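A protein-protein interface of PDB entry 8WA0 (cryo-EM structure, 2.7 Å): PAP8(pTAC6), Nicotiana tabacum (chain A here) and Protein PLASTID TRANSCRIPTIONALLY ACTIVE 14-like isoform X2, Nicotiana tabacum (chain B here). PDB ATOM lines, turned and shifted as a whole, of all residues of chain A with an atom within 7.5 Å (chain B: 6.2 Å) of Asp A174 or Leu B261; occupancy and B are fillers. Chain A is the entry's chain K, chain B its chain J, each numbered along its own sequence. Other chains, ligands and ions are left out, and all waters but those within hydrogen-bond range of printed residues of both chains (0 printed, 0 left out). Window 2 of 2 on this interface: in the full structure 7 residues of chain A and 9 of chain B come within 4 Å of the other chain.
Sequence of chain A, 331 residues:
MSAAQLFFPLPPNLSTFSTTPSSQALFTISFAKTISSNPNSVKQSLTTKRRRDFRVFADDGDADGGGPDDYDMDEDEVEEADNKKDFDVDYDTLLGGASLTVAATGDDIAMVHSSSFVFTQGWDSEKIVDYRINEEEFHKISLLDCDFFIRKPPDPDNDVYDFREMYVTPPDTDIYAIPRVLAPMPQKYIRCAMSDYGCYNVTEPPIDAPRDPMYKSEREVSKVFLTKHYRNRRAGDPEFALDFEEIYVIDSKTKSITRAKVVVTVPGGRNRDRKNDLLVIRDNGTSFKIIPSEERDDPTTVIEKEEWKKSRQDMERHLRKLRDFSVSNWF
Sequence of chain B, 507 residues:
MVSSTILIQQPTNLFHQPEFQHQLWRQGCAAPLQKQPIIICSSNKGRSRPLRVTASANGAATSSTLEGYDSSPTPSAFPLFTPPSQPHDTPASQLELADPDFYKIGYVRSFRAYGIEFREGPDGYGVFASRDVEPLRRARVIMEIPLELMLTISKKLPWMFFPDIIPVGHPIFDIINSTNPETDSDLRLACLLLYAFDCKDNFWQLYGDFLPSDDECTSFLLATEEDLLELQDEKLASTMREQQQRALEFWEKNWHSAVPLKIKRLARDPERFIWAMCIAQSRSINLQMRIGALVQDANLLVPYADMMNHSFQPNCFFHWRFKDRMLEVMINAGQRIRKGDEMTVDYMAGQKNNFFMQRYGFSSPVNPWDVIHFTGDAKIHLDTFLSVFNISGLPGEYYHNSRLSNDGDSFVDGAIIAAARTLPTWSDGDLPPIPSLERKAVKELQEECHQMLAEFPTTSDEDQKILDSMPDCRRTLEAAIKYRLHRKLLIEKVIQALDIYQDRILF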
ATOM      1  N   TYR A 131      10.814 -13.663   2.101  1.00  0.00           N
ATOM      2  CA  TYR A 131      12.127 -13.711   2.692  1.00  0.00           C
ATOM      3  C   TYR A 131      13.134 -13.393   1.605  1.00  0.00           C
ATOM      4  O   TYR A 131      12.921 -13.767   0.456  1.00  0.00           O
ATOM      5  CB  TYR A 131      12.404 -15.055   3.351  1.00  0.00           C
ATOM      6  CG  TYR A 131      12.101 -16.303   2.561  1.00  0.00           C
ATOM      7  CD1 TYR A 131      13.048 -16.860   1.717  1.00  0.00           C
ATOM      8  CD2 TYR A 131      10.895 -16.965   2.718  1.00  0.00           C
ATOM      9  CE1 TYR A 131      12.783 -18.016   1.013  1.00  0.00           C
ATOM     10  CE2 TYR A 131      10.622 -18.125   2.023  1.00  0.00           C
ATOM     11  CZ  TYR A 131      11.570 -18.644   1.171  1.00  0.00           C
ATOM     12  OH  TYR A 131      11.300 -19.798   0.474  1.00  0.00           O
ATOM     13  N   ARG A 132      14.218 -12.695   1.920  1.00  0.00           N
ATOM     14  CA  ARG A 132      15.191 -12.465   0.884  1.00  0.00           C
ATOM     15  C   ARG A 132      16.304 -13.451   0.984  1.00  0.00           C
ATOM     16  O   ARG A 132      16.985 -13.512   1.994  1.00  0.00           O
ATOM     17  CB  ARG A 132      15.700 -11.039   0.899  1.00  0.00           C
ATOM     18  CG  ARG A 132      15.923 -10.422   2.268  1.00  0.00           C
ATOM     19  CD  ARG A 132      17.021  -9.368   2.207  1.00  0.00           C
ATOM     20  NE  ARG A 132      16.888  -8.477   1.054  1.00  0.00           N
ATOM     21  CZ  ARG A 132      16.313  -7.280   1.090  1.00  0.00           C
ATOM     22  NH1 ARG A 132      15.814  -6.812   2.224  1.00  0.00           N
ATOM     23  NH2 ARG A 132      16.241  -6.547  -0.010  1.00  0.00           N
ATOM     24  N   ILE A 133      16.510 -14.229  -0.055  1.00  0.00           N
ATOM     25  CA  ILE A 133      17.495 -15.280  -0.032  1.00  0.00           C
ATOM     26  C   ILE A 133      18.913 -14.841  -0.144  1.00  0.00           C
ATOM     27  O   ILE A 133      19.186 -13.699  -0.472  1.00  0.00           O
ATOM     28  CB  ILE A 133      17.216 -16.228  -1.178  1.00  0.00           C
ATOM     29  CG1 ILE A 133      17.096 -15.461  -2.491  1.00  0.00           C
ATOM     30  CG2 ILE A 133      15.927 -16.986  -0.933  1.00  0.00           C
ATOM     31  CD1 ILE A 133      16.765 -16.337  -3.678  1.00  0.00           C
ATOM     32  N   GLU A 135      21.957 -15.204  -2.249  1.00  0.00           N
ATOM     33  CA  GLU A 135      22.121 -15.689  -3.565  1.00  0.00           C
ATOM     34  C   GLU A 135      23.470 -16.204  -3.782  1.00  0.00           C
ATOM     35  O   GLU A 135      23.771 -16.706  -4.849  1.00  0.00           O
ATOM     36  CB  GLU A 135      21.831 -14.584  -4.547  1.00  0.00           C
ATOM     37  CG  GLU A 135      20.376 -14.207  -4.660  1.00  0.00           C
ATOM     38  CD  GLU A 135      20.151 -13.233  -5.789  1.00  0.00           C
ATOM     39  OE1 GLU A 135      19.052 -13.250  -6.369  1.00  0.00           O
ATOM     40  OE2 GLU A 135      21.080 -12.465  -6.109  1.00  0.00           O
ATOM     41  N   LYS A 140      22.554 -18.898 -10.601  1.00  0.00           N
ATOM     42  CA  LYS A 140      21.692 -17.929 -11.249  1.00  0.00           C
ATOM     43  C   LYS A 140      21.775 -18.138 -12.729  1.00  0.00           C
ATOM     44  O   LYS A 140      22.856 -18.153 -13.298  1.00  0.00           O
ATOM     45  CB  LYS A 140      22.121 -16.510 -10.921  1.00  0.00           C
ATOM     46  CG  LYS A 140      21.322 -15.440 -11.639  1.00  0.00           C
ATOM     47  CD  LYS A 140      21.792 -14.053 -11.252  1.00  0.00           C
ATOM     48  CE  LYS A 140      20.973 -12.992 -11.964  1.00  0.00           C
ATOM     49  NZ  LYS A 140      21.388 -11.616 -11.579  1.00  0.00           N
ATOM     50  N   ASP A 147      15.007 -14.387 -14.254  1.00  0.00           N
ATOM     51  CA  ASP A 147      16.218 -14.931 -13.685  1.00  0.00           C
ATOM     52  C   ASP A 147      15.765 -16.128 -12.913  1.00  0.00           C
ATOM     53  O   ASP A 147      14.799 -16.043 -12.183  1.00  0.00           O
ATOM     54  CB  ASP A 147      16.875 -13.942 -12.756  1.00  0.00           C
ATOM     55  CG  ASP A 147      17.556 -12.814 -13.490  1.00  0.00           C
ATOM     56  OD1 ASP A 147      17.884 -12.995 -14.676  1.00  0.00           O
ATOM     57  OD2 ASP A 147      17.776 -11.751 -12.876  1.00  0.00           O
ATOM     58  N   PHE A 149      16.619 -19.263 -10.244  1.00  0.00           N
ATOM     59  CA  PHE A 149      17.560 -19.649  -9.223  1.00  0.00           C
ATOM     60  C   PHE A 149      17.326 -21.071  -8.764  1.00  0.00           C
ATOM     61  O   PHE A 149      16.215 -21.422  -8.424  1.00  0.00           O
ATOM     62  CB  PHE A 149      17.420 -18.703  -8.050  1.00  0.00           C
ATOM     63  CG  PHE A 149      17.665 -17.274  -8.392  1.00  0.00           C
ATOM     64  CD1 PHE A 149      18.949 -16.781  -8.442  1.00  0.00           C
ATOM     65  CD2 PHE A 149      16.610 -16.420  -8.646  1.00  0.00           C
ATOM     66  CE1 PHE A 149      19.180 -15.462  -8.754  1.00  0.00           C
ATOM     67  CE2 PHE A 149      16.834 -15.103  -8.961  1.00  0.00           C
ATOM     68  CZ  PHE A 149      18.121 -14.622  -9.017  1.00  0.00           C
ATOM     69  N   THR A 169      12.755 -14.443 -10.782  1.00  0.00           N
ATOM     70  CA  THR A 169      12.660 -12.998 -10.549  1.00  0.00           C
ATOM     71  C   THR A 169      12.604 -12.109 -11.815  1.00  0.00           C
ATOM     72  O   THR A 169      13.272 -12.430 -12.787  1.00  0.00           O
ATOM     73  CB  THR A 169      13.817 -12.519  -9.686  1.00  0.00           C
ATOM     74  OG1 THR A 169      14.082 -13.498  -8.681  1.00  0.00           O
ATOM     75  CG2 THR A 169      13.448 -11.248  -9.005  1.00  0.00           C
ATOM     76  N   PRO A 170      11.804 -10.998 -11.832  1.00  0.00           N
ATOM     77  CA  PRO A 170      11.806 -10.119 -12.980  1.00  0.00           C
ATOM     78  C   PRO A 170      13.217  -9.715 -13.234  1.00  0.00           C
ATOM     79  O   PRO A 170      13.993  -9.643 -12.289  1.00  0.00           O
ATOM     80  CB  PRO A 170      11.020  -8.955 -12.454  1.00  0.00           C
ATOM     81  CG  PRO A 170       9.983  -9.579 -11.590  1.00  0.00           C
ATOM     82  CD  PRO A 170      10.493 -10.934 -11.185  1.00  0.00           C
ATOM     83  N   PRO A 171      13.580  -9.417 -14.478  1.00  0.00           N
ATOM     84  CA  PRO A 171      15.006  -9.203 -14.710  1.00  0.00           C
ATOM     85  C   PRO A 171      15.730  -8.159 -13.883  1.00  0.00           C
ATOM     86  O   PRO A 171      15.270  -7.023 -13.821  1.00  0.00           O
ATOM     87  CB  PRO A 171      15.062  -8.851 -16.157  1.00  0.00           C
ATOM     88  CG  PRO A 171      13.701  -8.369 -16.520  1.00  0.00           C
ATOM     89  CD  PRO A 171      12.773  -9.168 -15.677  1.00  0.00           C
ATOM     90  N   ASP A 172      16.838  -8.532 -13.242  1.00  0.00           N
ATOM     91  CA  ASP A 172      17.637  -7.620 -12.400  1.00  0.00           C
ATOM     92  C   ASP A 172      16.884  -6.871 -11.327  1.00  0.00           C
ATOM     93  O   ASP A 172      17.169  -5.717 -11.069  1.00  0.00           O
ATOM     94  CB  ASP A 172      18.481  -6.671 -13.235  1.00  0.00           C
ATOM     95  CG  ASP A 172      19.783  -6.301 -12.554  1.00  0.00           C
ATOM     96  OD1 ASP A 172      20.058  -6.845 -11.465  1.00  0.00           O
ATOM     97  OD2 ASP A 172      20.531  -5.466 -13.106  1.00  0.00           O
ATOM     98  N   THR A 173      15.937  -7.516 -10.685  1.00  0.00           N
ATOM     99  CA  THR A 173      15.164  -6.899  -9.649  1.00  0.00           C
ATOM    100  C   THR A 173      15.082  -7.917  -8.592  1.00  0.00           C
ATOM    101  O   THR A 173      15.514  -9.028  -8.784  1.00  0.00           O
ATOM    102  CB  THR A 173      13.735  -6.680 -10.077  1.00  0.00           C
ATOM    103  N   ASP A 174      14.821  -7.590  -7.336  1.00  0.00           N
ATOM    104  CA  ASP A 174      14.933  -8.606  -6.251  1.00  0.00           C
ATOM    105  C   ASP A 174      13.753  -9.045  -5.422  1.00  0.00           C
ATOM    106  O   ASP A 174      13.903  -9.273  -4.239  1.00  0.00           O
ATOM    107  CB  ASP A 174      15.992  -8.211  -5.245  1.00  0.00           C
ATOM    108  CG  ASP A 174      17.295  -8.944  -5.454  1.00  0.00           C
ATOM    109  OD1 ASP A 174      17.509  -9.492  -6.555  1.00  0.00           O
ATOM    110  OD2 ASP A 174      18.108  -8.982  -4.509  1.00  0.00           O
ATOM    111  N   ILE A 175      12.588  -9.174  -6.012  1.00  0.00           N
ATOM    112  CA  ILE A 175      11.449  -9.672  -5.309  1.00  0.00           C
ATOM    113  C   ILE A 175      11.325 -11.098  -5.762  1.00  0.00           C
ATOM    114  O   ILE A 175      10.959 -11.338  -6.904  1.00  0.00           O
ATOM    115  CB  ILE A 175      10.239  -8.934  -5.829  1.00  0.00           C
ATOM    116  CG1 ILE A 175      10.543  -7.442  -5.951  1.00  0.00           C
ATOM    117  CG2 ILE A 175       9.041  -9.170  -4.920  1.00  0.00           C
ATOM    118  CD1 ILE A 175       9.417  -6.639  -6.560  1.00  0.00           C
ATOM    119  N   TYR A 176      11.589 -12.062  -4.903  1.00  0.00           N
ATOM    120  CA  TYR A 176      11.601 -13.450  -5.319  1.00  0.00           C
ATOM    121  C   TYR A 176      10.271 -14.174  -5.373  1.00  0.00           C
ATOM    122  O   TYR A 176       9.391 -13.873  -4.585  1.00  0.00           O
ATOM    123  CB  TYR A 176      12.579 -14.179  -4.472  1.00  0.00           C
ATOM    124  CG  TYR A 176      13.927 -13.537  -4.370  1.00  0.00           C
ATOM    125  CD1 TYR A 176      14.860 -13.693  -5.370  1.00  0.00           C
ATOM    126  CD2 TYR A 176      14.278 -12.791  -3.260  1.00  0.00           C
ATOM    127  CE1 TYR A 176      16.100 -13.113  -5.280  1.00  0.00           C
ATOM    128  CE2 TYR A 176      15.520 -12.205  -3.160  1.00  0.00           C
ATOM    129  CZ  TYR A 176      16.426 -12.373  -4.174  1.00  0.00           C
ATOM    130  OH  TYR A 176      17.666 -11.801  -4.080  1.00  0.00           O
ATOM    131  N   ALA A 177      10.099 -15.110  -6.299  1.00  0.00           N
ATOM    132  CA  ALA A 177       8.824 -15.820  -6.468  1.00  0.00           C
ATOM    133  C   ALA A 177       8.934 -17.293  -6.896  1.00  0.00           C
ATOM    134  O   ALA A 177       9.934 -17.668  -7.461  1.00  0.00           O
ATOM    135  CB  ALA A 177       7.990 -15.086  -7.466  1.00  0.00           C
ATOM    136  N   VAL B 259      18.319  -1.714   1.845  1.00  0.00           N
ATOM    137  CA  VAL B 259      18.649  -1.269   0.506  1.00  0.00           C
ATOM    138  C   VAL B 259      18.527  -2.393  -0.494  1.00  0.00           C
ATOM    139  O   VAL B 259      18.816  -3.540  -0.176  1.00  0.00           O
ATOM    140  CB  VAL B 259      20.028  -0.606   0.531  1.00  0.00           C
ATOM    141  N   PRO B 260      18.052  -2.085  -1.706  1.00  0.00           N
ATOM    142  CA  PRO B 260      17.959  -3.097  -2.751  1.00  0.00           C
ATOM    143  C   PRO B 260      19.315  -3.633  -3.106  1.00  0.00           C
ATOM    144  O   PRO B 260      20.274  -2.891  -3.015  1.00  0.00           O
ATOM    145  CB  PRO B 260      17.333  -2.348  -3.900  1.00  0.00           C
ATOM    146  CG  PRO B 260      17.268  -0.915  -3.514  1.00  0.00           C
ATOM    147  CD  PRO B 260      17.263  -0.894  -2.032  1.00  0.00           C
ATOM    148  N   LEU B 261      19.432  -4.870  -3.519  1.00  0.00           N
ATOM    149  CA  LEU B 261      20.746  -5.458  -3.714  1.00  0.00           C
ATOM    150  C   LEU B 261      21.624  -4.768  -4.728  1.00  0.00           C
ATOM    151  O   LEU B 261      22.842  -4.794  -4.603  1.00  0.00           O
ATOM    152  CB  LEU B 261      20.658  -6.941  -4.018  1.00  0.00           C
ATOM    153  CG  LEU B 261      21.930  -7.779  -3.975  1.00  0.00           C
ATOM    154  CD1 LEU B 261      22.483  -7.828  -2.561  1.00  0.00           C
ATOM    155  CD2 LEU B 261      21.655  -9.175  -4.497  1.00  0.00           C
ATOM    156  N   LYS B 262      21.037  -4.125  -5.718  1.00  0.00           N
ATOM    157  CA  LYS B 262      21.813  -3.416  -6.698  1.00  0.00           C
ATOM    158  C   LYS B 262      22.638  -2.391  -5.987  1.00  0.00           C
ATOM    159  O   LYS B 262      23.817  -2.274  -6.260  1.00  0.00           O
ATOM    160  CB  LYS B 262      20.874  -2.657  -7.601  1.00  0.00           C
ATOM    161  CG  LYS B 262      19.591  -3.334  -8.003  1.00  0.00           C
ATOM    162  CD  LYS B 262      18.784  -2.332  -8.800  1.00  0.00           C
ATOM    163  CE  LYS B 262      17.484  -2.909  -9.304  1.00  0.00           C
ATOM    164  NZ  LYS B 262      16.772  -1.911 -10.144  1.00  0.00           N
ATOM    165  N   ILE B 263      22.052  -1.650  -5.059  1.00  0.00           N
ATOM    166  CA  ILE B 263      22.791  -0.717  -4.264  1.00  0.00           C
ATOM    167  C   ILE B 263      23.777  -1.374  -3.330  1.00  0.00           C
ATOM    168  O   ILE B 263      24.905  -0.927  -3.219  1.00  0.00           O
ATOM    169  CB  ILE B 263      21.888   0.250  -3.522  1.00  0.00           C
ATOM    170  CG1 ILE B 263      21.093   1.101  -4.485  1.00  0.00           C
ATOM    171  CG2 ILE B 263      22.691   1.187  -2.638  1.00  0.00           C
ATOM    172  CD1 ILE B 263      20.475   2.286  -3.784  1.00  0.00           C
ATOM    173  N   LYS B 264      23.407  -2.461  -2.695  1.00  0.00           N
ATOM    174  CA  LYS B 264      24.305  -3.081  -1.743  1.00  0.00           C
ATOM    175  C   LYS B 264      25.565  -3.613  -2.332  1.00  0.00           C
ATOM    176  O   LYS B 264      26.618  -3.461  -1.750  1.00  0.00           O
ATOM    177  CB  LYS B 264      23.634  -4.156  -0.929  1.00  0.00           C
ATOM    178  CG  LYS B 264      24.309  -4.459   0.392  1.00  0.00           C
ATOM    179  CD  LYS B 264      23.493  -5.456   1.192  1.00  0.00           C
ATOM    180  CE  LYS B 264      22.081  -4.950   1.446  1.00  0.00           C
ATOM    181  NZ  LYS B 264      22.058  -3.777   2.366  1.00  0.00           N
ATOM    182  N   ARG B 265      25.494  -4.216  -3.492  1.00  0.00           N
ATOM    183  CA  ARG B 265      26.660  -4.815  -4.056  1.00  0.00           C
ATOM    184  C   ARG B 265      27.730  -3.791  -4.300  1.00  0.00           C
ATOM    185  O   ARG B 265      28.911  -4.091  -4.194  1.00  0.00           O
ATOM    186  CB  ARG B 265      26.344  -5.622  -5.316  1.00  0.00           C
ATOM    187  CG  ARG B 265      25.456  -5.016  -6.377  1.00  0.00           C
ATOM    188  CD  ARG B 265      25.492  -5.947  -7.577  1.00  0.00           C
ATOM    189  NE  ARG B 265      24.667  -5.516  -8.695  1.00  0.00           N
ATOM    190  CZ  ARG B 265      23.476  -6.022  -8.984  1.00  0.00           C
ATOM    191  NH1 ARG B 265      22.964  -6.983  -8.236  1.00  0.00           N
ATOM    192  NH2 ARG B 265      22.799  -5.573 -10.026  1.00  0.00           N
ATOM    193  N   LEU B 266      27.343  -2.582  -4.640  1.00  0.00           N
ATOM    194  CA  LEU B 266      28.312  -1.598  -4.993  1.00  0.00           C
ATOM    195  C   LEU B 266      29.255  -1.302  -3.844  1.00  0.00           C
ATOM    196  O   LEU B 266      30.456  -1.225  -4.072  1.00  0.00           O
ATOM    197  CB  LEU B 266      27.590  -0.378  -5.532  1.00  0.00           C
ATOM    198  CG  LEU B 266      26.628  -0.488  -6.696  1.00  0.00           C
ATOM    199  CD1 LEU B 266      25.955   0.855  -6.882  1.00  0.00           C
ATOM    200  CD2 LEU B 266      27.364  -0.907  -7.954  1.00  0.00           C
ATOM    201  N   ARG B 268      29.608  -3.041  -0.182  1.00  0.00           N
ATOM    202  CA  ARG B 268      29.299  -3.902   0.949  1.00  0.00           C
ATOM    203  C   ARG B 268      29.980  -3.550   2.239  1.00  0.00           C
ATOM    204  O   ARG B 268      29.338  -3.555   3.268  1.00  0.00           O
ATOM    205  CB  ARG B 268      29.618  -5.337   0.573  1.00  0.00           C
ATOM    206  CG  ARG B 268      29.167  -5.703  -0.829  1.00  0.00           C
ATOM    207  CD  ARG B 268      28.950  -7.196  -0.978  1.00  0.00           C
ATOM    208  NE  ARG B 268      27.886  -7.680  -0.105  1.00  0.00           N
ATOM    209  CZ  ARG B 268      26.606  -7.758  -0.452  1.00  0.00           C
ATOM    210  NH1 ARG B 268      26.215  -7.386  -1.662  1.00  0.00           N
ATOM    211  NH2 ARG B 268      25.711  -8.215   0.414  1.00  0.00           N
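Among the printed residues, pairs that only touch across the chains: Asp A174 with Leu B261 (3.3 Å), Asp A172 with Lys B262 (3.3 Å), Glu A135 with Leu B261 (3.7 Å) and Arg A132 with Val B259 (3.96 Å).
The guanidinium group of Arg B265 lies within salt-bridge range of the side-chain carboxylate of Asp A172, 3.3 Å away.
Hydrophobic or aromatic side chains of chain B within 4 Å of the printed part of chain A: Leu B261.
Along chain B the printed residues that touch a printed residue of chain A span positions 259 to 265.
Printed residues of chain A that touch a printed residue of chain B: Arg A132, Glu A135, Asp A172 and Asp A174.
Among the printed residues, Asp or Glu carboxylates within 4 Å of a Lys or Arg side-chain nitrogen of the other chain: Asp A172 with Arg B265 (3.3 Å).
Printed residues of chain B within 4 Å of Glu A135: Leu B261.
Printed residues of chain B within 4 Å of Asp A172: Lys B262 (3.3 Å) and Arg B265 (3.3 Å).
Of the printed residues of chain B, Asp A174 touches Leu B261 (3.3 Å).
Printed residues of chain A within 4 Å of Val B259: Arg A132.
Leu B261 touches just these residues of chain A: Glu A135 and Asp A174.
Of the printed residues of chain A, Lys B262 touches Asp A172.
The nearest residue of chain A that does not touch Leu B261 is Tyr A176 (4.8 Å).
The nearest printed residue of chain B that does not touch Asp A172 is Leu B261 (7.2 Å).
OH of Tyr A176 sits at hydrogen-bond distance from OE1 of Glu A135, 3.0 Å away.
The backbone NH (N) of Asp A172 sits at hydrogen-bond distance from the side-chain carboxylate (OD2) of Asp A147 (3.4 Å).
The side-chain carboxylate of Asp A174 is in hydrogen-bond range of the side-chain hydroxyl of Tyr A176 (2.9 Å).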
